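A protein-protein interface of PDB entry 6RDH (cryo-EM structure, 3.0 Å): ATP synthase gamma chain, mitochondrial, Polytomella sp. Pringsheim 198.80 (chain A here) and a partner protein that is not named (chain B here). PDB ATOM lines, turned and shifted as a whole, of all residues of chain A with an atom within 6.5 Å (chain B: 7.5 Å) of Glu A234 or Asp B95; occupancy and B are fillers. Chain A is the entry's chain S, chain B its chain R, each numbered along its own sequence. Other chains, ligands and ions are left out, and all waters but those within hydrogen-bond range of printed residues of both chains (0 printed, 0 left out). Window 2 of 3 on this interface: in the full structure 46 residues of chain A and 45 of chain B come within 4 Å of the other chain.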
ATOM      1  N   ASP A 232       8.938  -1.607 -22.090  1.00  0.00           N
ATOM      2  CA  ASP A 232       8.414  -2.806 -22.716  1.00  0.00           C
ATOM      3  C   ASP A 232       7.382  -3.435 -21.793  1.00  0.00           C
ATOM      4  O   ASP A 232       7.731  -3.971 -20.741  1.00  0.00           O
ATOM      5  CB  ASP A 232       9.549  -3.789 -22.999  1.00  0.00           C
ATOM      6  CG  ASP A 232       9.322  -4.602 -24.248  1.00  0.00           C
ATOM      7  OD1 ASP A 232       9.871  -5.718 -24.333  1.00  0.00           O
ATOM      8  OD2 ASP A 232       8.591  -4.131 -25.141  1.00  0.00           O
ATOM      9  N   ILE A 233       6.121  -3.384 -22.193  1.00  0.00           N
ATOM     10  CA  ILE A 233       5.043  -3.874 -21.345  1.00  0.00           C
ATOM     11  C   ILE A 233       5.018  -5.388 -21.431  1.00  0.00           C
ATOM     12  O   ILE A 233       4.980  -5.960 -22.524  1.00  0.00           O
ATOM     13  CB  ILE A 233       3.698  -3.276 -21.764  1.00  0.00           C
ATOM     14  CG1 ILE A 233       3.801  -1.763 -21.758  1.00  0.00           C
ATOM     15  CG2 ILE A 233       2.607  -3.733 -20.835  1.00  0.00           C
ATOM     16  CD1 ILE A 233       4.104  -1.184 -20.414  1.00  0.00           C
ATOM     17  N   GLU A 234       5.053  -6.041 -20.280  1.00  0.00           N
ATOM     18  CA  GLU A 234       5.130  -7.489 -20.202  1.00  0.00           C
ATOM     19  C   GLU A 234       3.918  -8.047 -19.473  1.00  0.00           C
ATOM     20  O   GLU A 234       4.026  -8.962 -18.667  1.00  0.00           O
ATOM     21  CB  GLU A 234       6.428  -7.908 -19.521  1.00  0.00           C
ATOM     22  CG  GLU A 234       7.029  -9.213 -19.995  1.00  0.00           C
ATOM     23  CD  GLU A 234       6.757 -10.360 -19.051  1.00  0.00           C
ATOM     24  OE1 GLU A 234       6.525 -10.106 -17.851  1.00  0.00           O
ATOM     25  OE2 GLU A 234       6.799 -11.518 -19.501  1.00  0.00           O
ATOM     26  N   ALA A 235       2.749  -7.501 -19.749  1.00  0.00           N
ATOM     27  CA  ALA A 235       1.515  -7.978 -19.153  1.00  0.00           C
ATOM     28  C   ALA A 235       0.793  -8.879 -20.135  1.00  0.00           C
ATOM     29  O   ALA A 235       1.221  -9.066 -21.274  1.00  0.00           O
ATOM     30  CB  ALA A 235       0.621  -6.813 -18.746  1.00  0.00           C
ATOM     31  N   SER A 236      -0.325  -9.439 -19.683  1.00  0.00           N
ATOM     32  CA  SER A 236      -1.119 -10.290 -20.557  1.00  0.00           C
ATOM     33  C   SER A 236      -1.881  -9.455 -21.575  1.00  0.00           C
ATOM     34  O   SER A 236      -1.700  -9.605 -22.787  1.00  0.00           O
ATOM     35  CB  SER A 236      -2.083 -11.133 -19.729  1.00  0.00           C
ATOM     36  OG  SER A 236      -3.198 -10.361 -19.331  1.00  0.00           O
ATOM     37  N   HIS A 237      -2.727  -8.567 -21.098  1.00  0.00           N
ATOM     38  CA  HIS A 237      -3.589  -7.758 -21.941  1.00  0.00           C
ATOM     39  C   HIS A 237      -2.906  -6.424 -22.243  1.00  0.00           C
ATOM     40  O   HIS A 237      -1.689  -6.290 -22.106  1.00  0.00           O
ATOM     41  CB  HIS A 237      -4.953  -7.631 -21.280  1.00  0.00           C
ATOM     42  CG  HIS A 237      -5.708  -8.919 -21.253  1.00  0.00           C
ATOM     43  ND1 HIS A 237      -5.300 -10.002 -20.507  1.00  0.00           N
ATOM     44  CD2 HIS A 237      -6.831  -9.306 -21.896  1.00  0.00           C
ATOM     45  CE1 HIS A 237      -6.146 -10.999 -20.683  1.00  0.00           C
ATOM     46  NE2 HIS A 237      -7.085 -10.603 -21.522  1.00  0.00           N
ATOM     47  N   VAL A 242      -2.931  -2.634 -18.040  1.00  0.00           N
ATOM     48  CA  VAL A 242      -1.852  -2.687 -17.064  1.00  0.00           C
ATOM     49  C   VAL A 242      -1.734  -1.354 -16.340  1.00  0.00           C
ATOM     50  O   VAL A 242      -1.410  -1.317 -15.156  1.00  0.00           O
ATOM     51  CB  VAL A 242      -0.522  -3.137 -17.713  1.00  0.00           C
ATOM     52  CG1 VAL A 242       0.207  -2.034 -18.433  1.00  0.00           C
ATOM     53  CG2 VAL A 242       0.380  -3.708 -16.693  1.00  0.00           C
ATOM     54  N   LEU B  91      12.641 -12.694 -12.351  1.00  0.00           N
ATOM     55  CA  LEU B  91      11.307 -12.271 -11.988  1.00  0.00           C
ATOM     56  C   LEU B  91      10.258 -13.200 -12.576  1.00  0.00           C
ATOM     57  O   LEU B  91      10.428 -13.687 -13.692  1.00  0.00           O
ATOM     58  CB  LEU B  91      11.061 -10.852 -12.477  1.00  0.00           C
ATOM     59  CG  LEU B  91      11.871  -9.876 -11.651  1.00  0.00           C
ATOM     60  CD1 LEU B  91      11.951  -8.565 -12.348  1.00  0.00           C
ATOM     61  CD2 LEU B  91      11.204  -9.733 -10.323  1.00  0.00           C
ATOM     62  N   PRO B  92       9.178 -13.473 -11.859  1.00  0.00           N
ATOM     63  CA  PRO B  92       8.153 -14.402 -12.355  1.00  0.00           C
ATOM     64  C   PRO B  92       7.049 -13.716 -13.152  1.00  0.00           C
ATOM     65  O   PRO B  92       5.900 -13.616 -12.713  1.00  0.00           O
ATOM     66  CB  PRO B  92       7.628 -15.014 -11.060  1.00  0.00           C
ATOM     67  CG  PRO B  92       7.740 -13.909 -10.073  1.00  0.00           C
ATOM     68  CD  PRO B  92       8.887 -13.033 -10.489  1.00  0.00           C
ATOM     69  N   GLY B  93       7.385 -13.258 -14.357  1.00  0.00           N
ATOM     70  CA  GLY B  93       6.438 -12.540 -15.186  1.00  0.00           C
ATOM     71  C   GLY B  93       5.292 -13.414 -15.652  1.00  0.00           C
ATOM     72  O   GLY B  93       5.311 -14.636 -15.523  1.00  0.00           O
ATOM     73  N   VAL B  94       4.255 -12.769 -16.184  1.00  0.00           N
ATOM     74  CA  VAL B  94       3.059 -13.524 -16.538  1.00  0.00           C
ATOM     75  C   VAL B  94       3.276 -14.361 -17.787  1.00  0.00           C
ATOM     76  O   VAL B  94       2.616 -15.389 -17.968  1.00  0.00           O
ATOM     77  CB  VAL B  94       1.848 -12.597 -16.698  1.00  0.00           C
ATOM     78  CG1 VAL B  94       1.411 -12.074 -15.362  1.00  0.00           C
ATOM     79  CG2 VAL B  94       2.198 -11.454 -17.590  1.00  0.00           C
ATOM     80  N   ASP B  95       4.193 -13.953 -18.660  1.00  0.00           N
ATOM     81  CA  ASP B  95       4.531 -14.786 -19.801  1.00  0.00           C
ATOM     82  C   ASP B  95       5.467 -15.908 -19.395  1.00  0.00           C
ATOM     83  O   ASP B  95       5.438 -16.990 -19.989  1.00  0.00           O
ATOM     84  CB  ASP B  95       5.162 -13.936 -20.898  1.00  0.00           C
ATOM     85  CG  ASP B  95       4.243 -12.831 -21.372  1.00  0.00           C
ATOM     86  OD1 ASP B  95       4.752 -11.766 -21.771  1.00  0.00           O
ATOM     87  OD2 ASP B  95       3.010 -13.021 -21.333  1.00  0.00           O
ATOM     88  N   GLY B  96       6.274 -15.672 -18.381  1.00  0.00           N
ATOM     89  CA  GLY B  96       7.199 -16.665 -17.880  1.00  0.00           C
ATOM     90  C   GLY B  96       8.342 -15.986 -17.159  1.00  0.00           C
ATOM     91  O   GLY B  96       8.463 -14.769 -17.151  1.00  0.00           O
ATOM     92  N   TYR B  97       9.185 -16.814 -16.556  1.00  0.00           N
ATOM     93  CA  TYR B  97      10.295 -16.318 -15.757  1.00  0.00           C
ATOM     94  C   TYR B  97      11.324 -15.653 -16.651  1.00  0.00           C
ATOM     95  O   TYR B  97      11.839 -16.275 -17.580  1.00  0.00           O
ATOM     96  CB  TYR B  97      10.940 -17.461 -14.981  1.00  0.00           C
ATOM     97  CG  TYR B  97      10.144 -17.949 -13.803  1.00  0.00           C
ATOM     98  CD1 TYR B  97       9.088 -18.825 -13.974  1.00  0.00           C
ATOM     99  CD2 TYR B  97      10.457 -17.545 -12.518  1.00  0.00           C
ATOM    100  CE1 TYR B  97       8.358 -19.277 -12.903  1.00  0.00           C
ATOM    101  CE2 TYR B  97       9.733 -17.995 -11.439  1.00  0.00           C
ATOM    102  CZ  TYR B  97       8.684 -18.861 -11.640  1.00  0.00           C
ATOM    103  OH  TYR B  97       7.951 -19.322 -10.573  1.00  0.00           O
ATOM    104  N   PHE B  98      11.618 -14.391 -16.391  1.00  0.00           N
ATOM    105  CA  PHE B  98      12.686 -13.713 -17.098  1.00  0.00           C
ATOM    106  C   PHE B  98      13.726 -13.252 -16.096  1.00  0.00           C
ATOM    107  O   PHE B  98      13.479 -13.204 -14.894  1.00  0.00           O
ATOM    108  CB  PHE B  98      12.162 -12.537 -17.932  1.00  0.00           C
ATOM    109  CG  PHE B  98      11.547 -11.428 -17.133  1.00  0.00           C
ATOM    110  CD1 PHE B  98      10.227 -11.491 -16.724  1.00  0.00           C
ATOM    111  CD2 PHE B  98      12.273 -10.292 -16.841  1.00  0.00           C
ATOM    112  CE1 PHE B  98       9.669 -10.471 -16.011  1.00  0.00           C
ATOM    113  CE2 PHE B  98      11.716  -9.276 -16.131  1.00  0.00           C
ATOM    114  CZ  PHE B  98      10.418  -9.367 -15.713  1.00  0.00           C
ATOM    115  N   THR B 107      11.043  -1.759 -18.734  1.00  0.00           N
ATOM    116  CA  THR B 107      10.030  -2.799 -18.653  1.00  0.00           C
ATOM    117  C   THR B 107       9.045  -2.439 -17.553  1.00  0.00           C
ATOM    118  O   THR B 107       9.448  -1.918 -16.515  1.00  0.00           O
ATOM    119  CB  THR B 107      10.700  -4.153 -18.371  1.00  0.00           C
ATOM    120  OG1 THR B 107      11.574  -4.487 -19.452  1.00  0.00           O
ATOM    121  CG2 THR B 107       9.702  -5.266 -18.210  1.00  0.00           C
ATOM    122  N   ILE B 108       7.758  -2.653 -17.806  1.00  0.00           N
ATOM    123  CA  ILE B 108       6.737  -2.690 -16.766  1.00  0.00           C
ATOM    124  C   ILE B 108       6.142  -4.088 -16.813  1.00  0.00           C
ATOM    125  O   ILE B 108       5.188  -4.346 -17.552  1.00  0.00           O
ATOM    126  CB  ILE B 108       5.664  -1.619 -16.959  1.00  0.00           C
ATOM    127  CG1 ILE B 108       6.306  -0.245 -17.025  1.00  0.00           C
ATOM    128  CG2 ILE B 108       4.685  -1.646 -15.820  1.00  0.00           C
ATOM    129  CD1 ILE B 108       5.337   0.854 -17.324  1.00  0.00           C
ATOM    130  N   ALA B 109       6.697  -5.002 -16.034  1.00  0.00           N
ATOM    131  CA  ALA B 109       6.305  -6.399 -16.081  1.00  0.00           C
ATOM    132  C   ALA B 109       5.349  -6.710 -14.951  1.00  0.00           C
ATOM    133  O   ALA B 109       5.673  -6.489 -13.785  1.00  0.00           O
ATOM    134  CB  ALA B 109       7.520  -7.310 -15.984  1.00  0.00           C
ATOM    135  N   GLN B 110       4.183  -7.229 -15.295  1.00  0.00           N
ATOM    136  CA  GLN B 110       3.249  -7.712 -14.298  1.00  0.00           C
ATOM    137  C   GLN B 110       3.673  -9.109 -13.890  1.00  0.00           C
ATOM    138  O   GLN B 110       3.950  -9.948 -14.745  1.00  0.00           O
ATOM    139  CB  GLN B 110       1.822  -7.726 -14.833  1.00  0.00           C
ATOM    140  CG  GLN B 110       0.817  -8.143 -13.791  1.00  0.00           C
ATOM    141  CD  GLN B 110      -0.601  -8.079 -14.283  1.00  0.00           C
ATOM    142  OE1 GLN B 110      -0.891  -7.452 -15.296  1.00  0.00           O
ATOM    143  NE2 GLN B 110      -1.501  -8.733 -13.566  1.00  0.00           N
ATOM    144  N   LEU B 111       3.730  -9.353 -12.592  1.00  0.00           N
ATOM    145  CA  LEU B 111       4.298 -10.581 -12.071  1.00  0.00           C
ATOM    146  C   LEU B 111       3.214 -11.571 -11.687  1.00  0.00           C
ATOM    147  O   LEU B 111       2.251 -11.233 -11.000  1.00  0.00           O
ATOM    148  CB  LEU B 111       5.189 -10.300 -10.869  1.00  0.00           C
ATOM    149  CG  LEU B 111       6.387  -9.397 -11.123  1.00  0.00           C
ATOM    150  CD1 LEU B 111       7.266  -9.384  -9.908  1.00  0.00           C
ATOM    151  CD2 LEU B 111       7.149  -9.857 -12.330  1.00  0.00           C
ATOM    152  N   LYS B 112       3.387 -12.797 -12.151  1.00  0.00           N
ATOM    153  CA  LYS B 112       2.583 -13.927 -11.767  1.00  0.00           C
ATOM    154  C   LYS B 112       3.054 -14.368 -10.388  1.00  0.00           C
ATOM    155  O   LYS B 112       4.155 -14.013  -9.970  1.00  0.00           O
ATOM    156  CB  LYS B 112       2.746 -15.022 -12.826  1.00  0.00           C
ATOM    157  CG  LYS B 112       1.800 -16.197 -12.787  1.00  0.00           C
ATOM    158  CD  LYS B 112       1.951 -17.058 -14.017  1.00  0.00           C
ATOM    159  CE  LYS B 112       3.244 -17.839 -13.983  1.00  0.00           C
ATOM    160  NZ  LYS B 112       3.304 -18.822 -15.097  1.00  0.00           N
ATOM    161  N   ALA B 134       6.877  -5.230 -11.525  1.00  0.00           N
ATOM    162  CA  ALA B 134       8.326  -5.123 -11.504  1.00  0.00           C
ATOM    163  C   ALA B 134       8.718  -4.158 -12.602  1.00  0.00           C
ATOM    164  O   ALA B 134       8.581  -4.481 -13.777  1.00  0.00           O
ATOM    165  CB  ALA B 134       8.973  -6.481 -11.711  1.00  0.00           C
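The backbone NH of Glu A234 sits at hydrogen-bond distance from the backbone carbonyl oxygen of Ile B108, at 3.2 Å. O of Asp A232 lies within hydrogen-bond range of N of Ile B108. OE2 of Glu A234 sits close to OD1 of Asp B95 (3.1 Å).
The backbone carbonyl oxygen of Ala B109 is in hydrogen-bond range of the backbone NH of Ala B134. The backbone NH (N) of Val B94 is in hydrogen-bond range of the backbone carbonyl oxygen (O) of Gln B110 (3.2 Å). The side-chain hydroxyl (OG) of Ser A236 sits at hydrogen-bond distance from a ring nitrogen (ND1) of His A237 (2.4 Å). The backbone NH (N) of Leu B91 lies within hydrogen-bond range of the backbone carbonyl oxygen (O) of Phe B98.
Among the printed residues, pairs that only touch across the chains: Asp A232 with Thr B107, Ile A233 with Ile B108, Glu A234 with Gly B93, Glu A234 with Val B94, Glu A234 with Phe B98, Glu A234 with Ala B109, Glu A234 with Gln B110, Ala A235 with Val B94, Ala A235 with Gln B110 and Ser A236 with Val B94.
Of chain B, only Gly B93, Val B94, Asp B95, Phe B98, Ile B108, Ala B109 and Gln B110 come within 4 Å of Glu A234. Asp B95 touches just one residue of chain A: Glu A234. Printed residues of chain B within 4 Å of Asp A232: Thr B107 and Ile B108. Of the printed residues of chain A, Ala B109 touches Glu A234 (3.5 Å). Printed residues of chain A within 4 Å of Val B94: Glu A234 (3.3 Å), Ala A235 (3.9 Å) and Ser A236 (3.8 Å). Of the printed residues of chain B, Ile A233 touches Ile B108. Val A242 touches none of the printed residues of chain B. Leu B111 touches none of the printed residues of chain A. The nearest residue of chain A that does not touch Asp B95 is Ala A235 (4.3 Å). The nearest printed residue of chain A that does not touch Ile B108 is Ala A235 (4.6 Å).
Printed residues of chain A that touch a printed residue of chain B: Asp A232, Ile A233, Glu A234, Ala A235 and Ser A236. Hydrophobic or aromatic side chains of chain A that line the printed part of chain B: Ile A233 and Ala A235. Of the 15 printed residues of chain B, 8 touch a printed residue of chain A.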
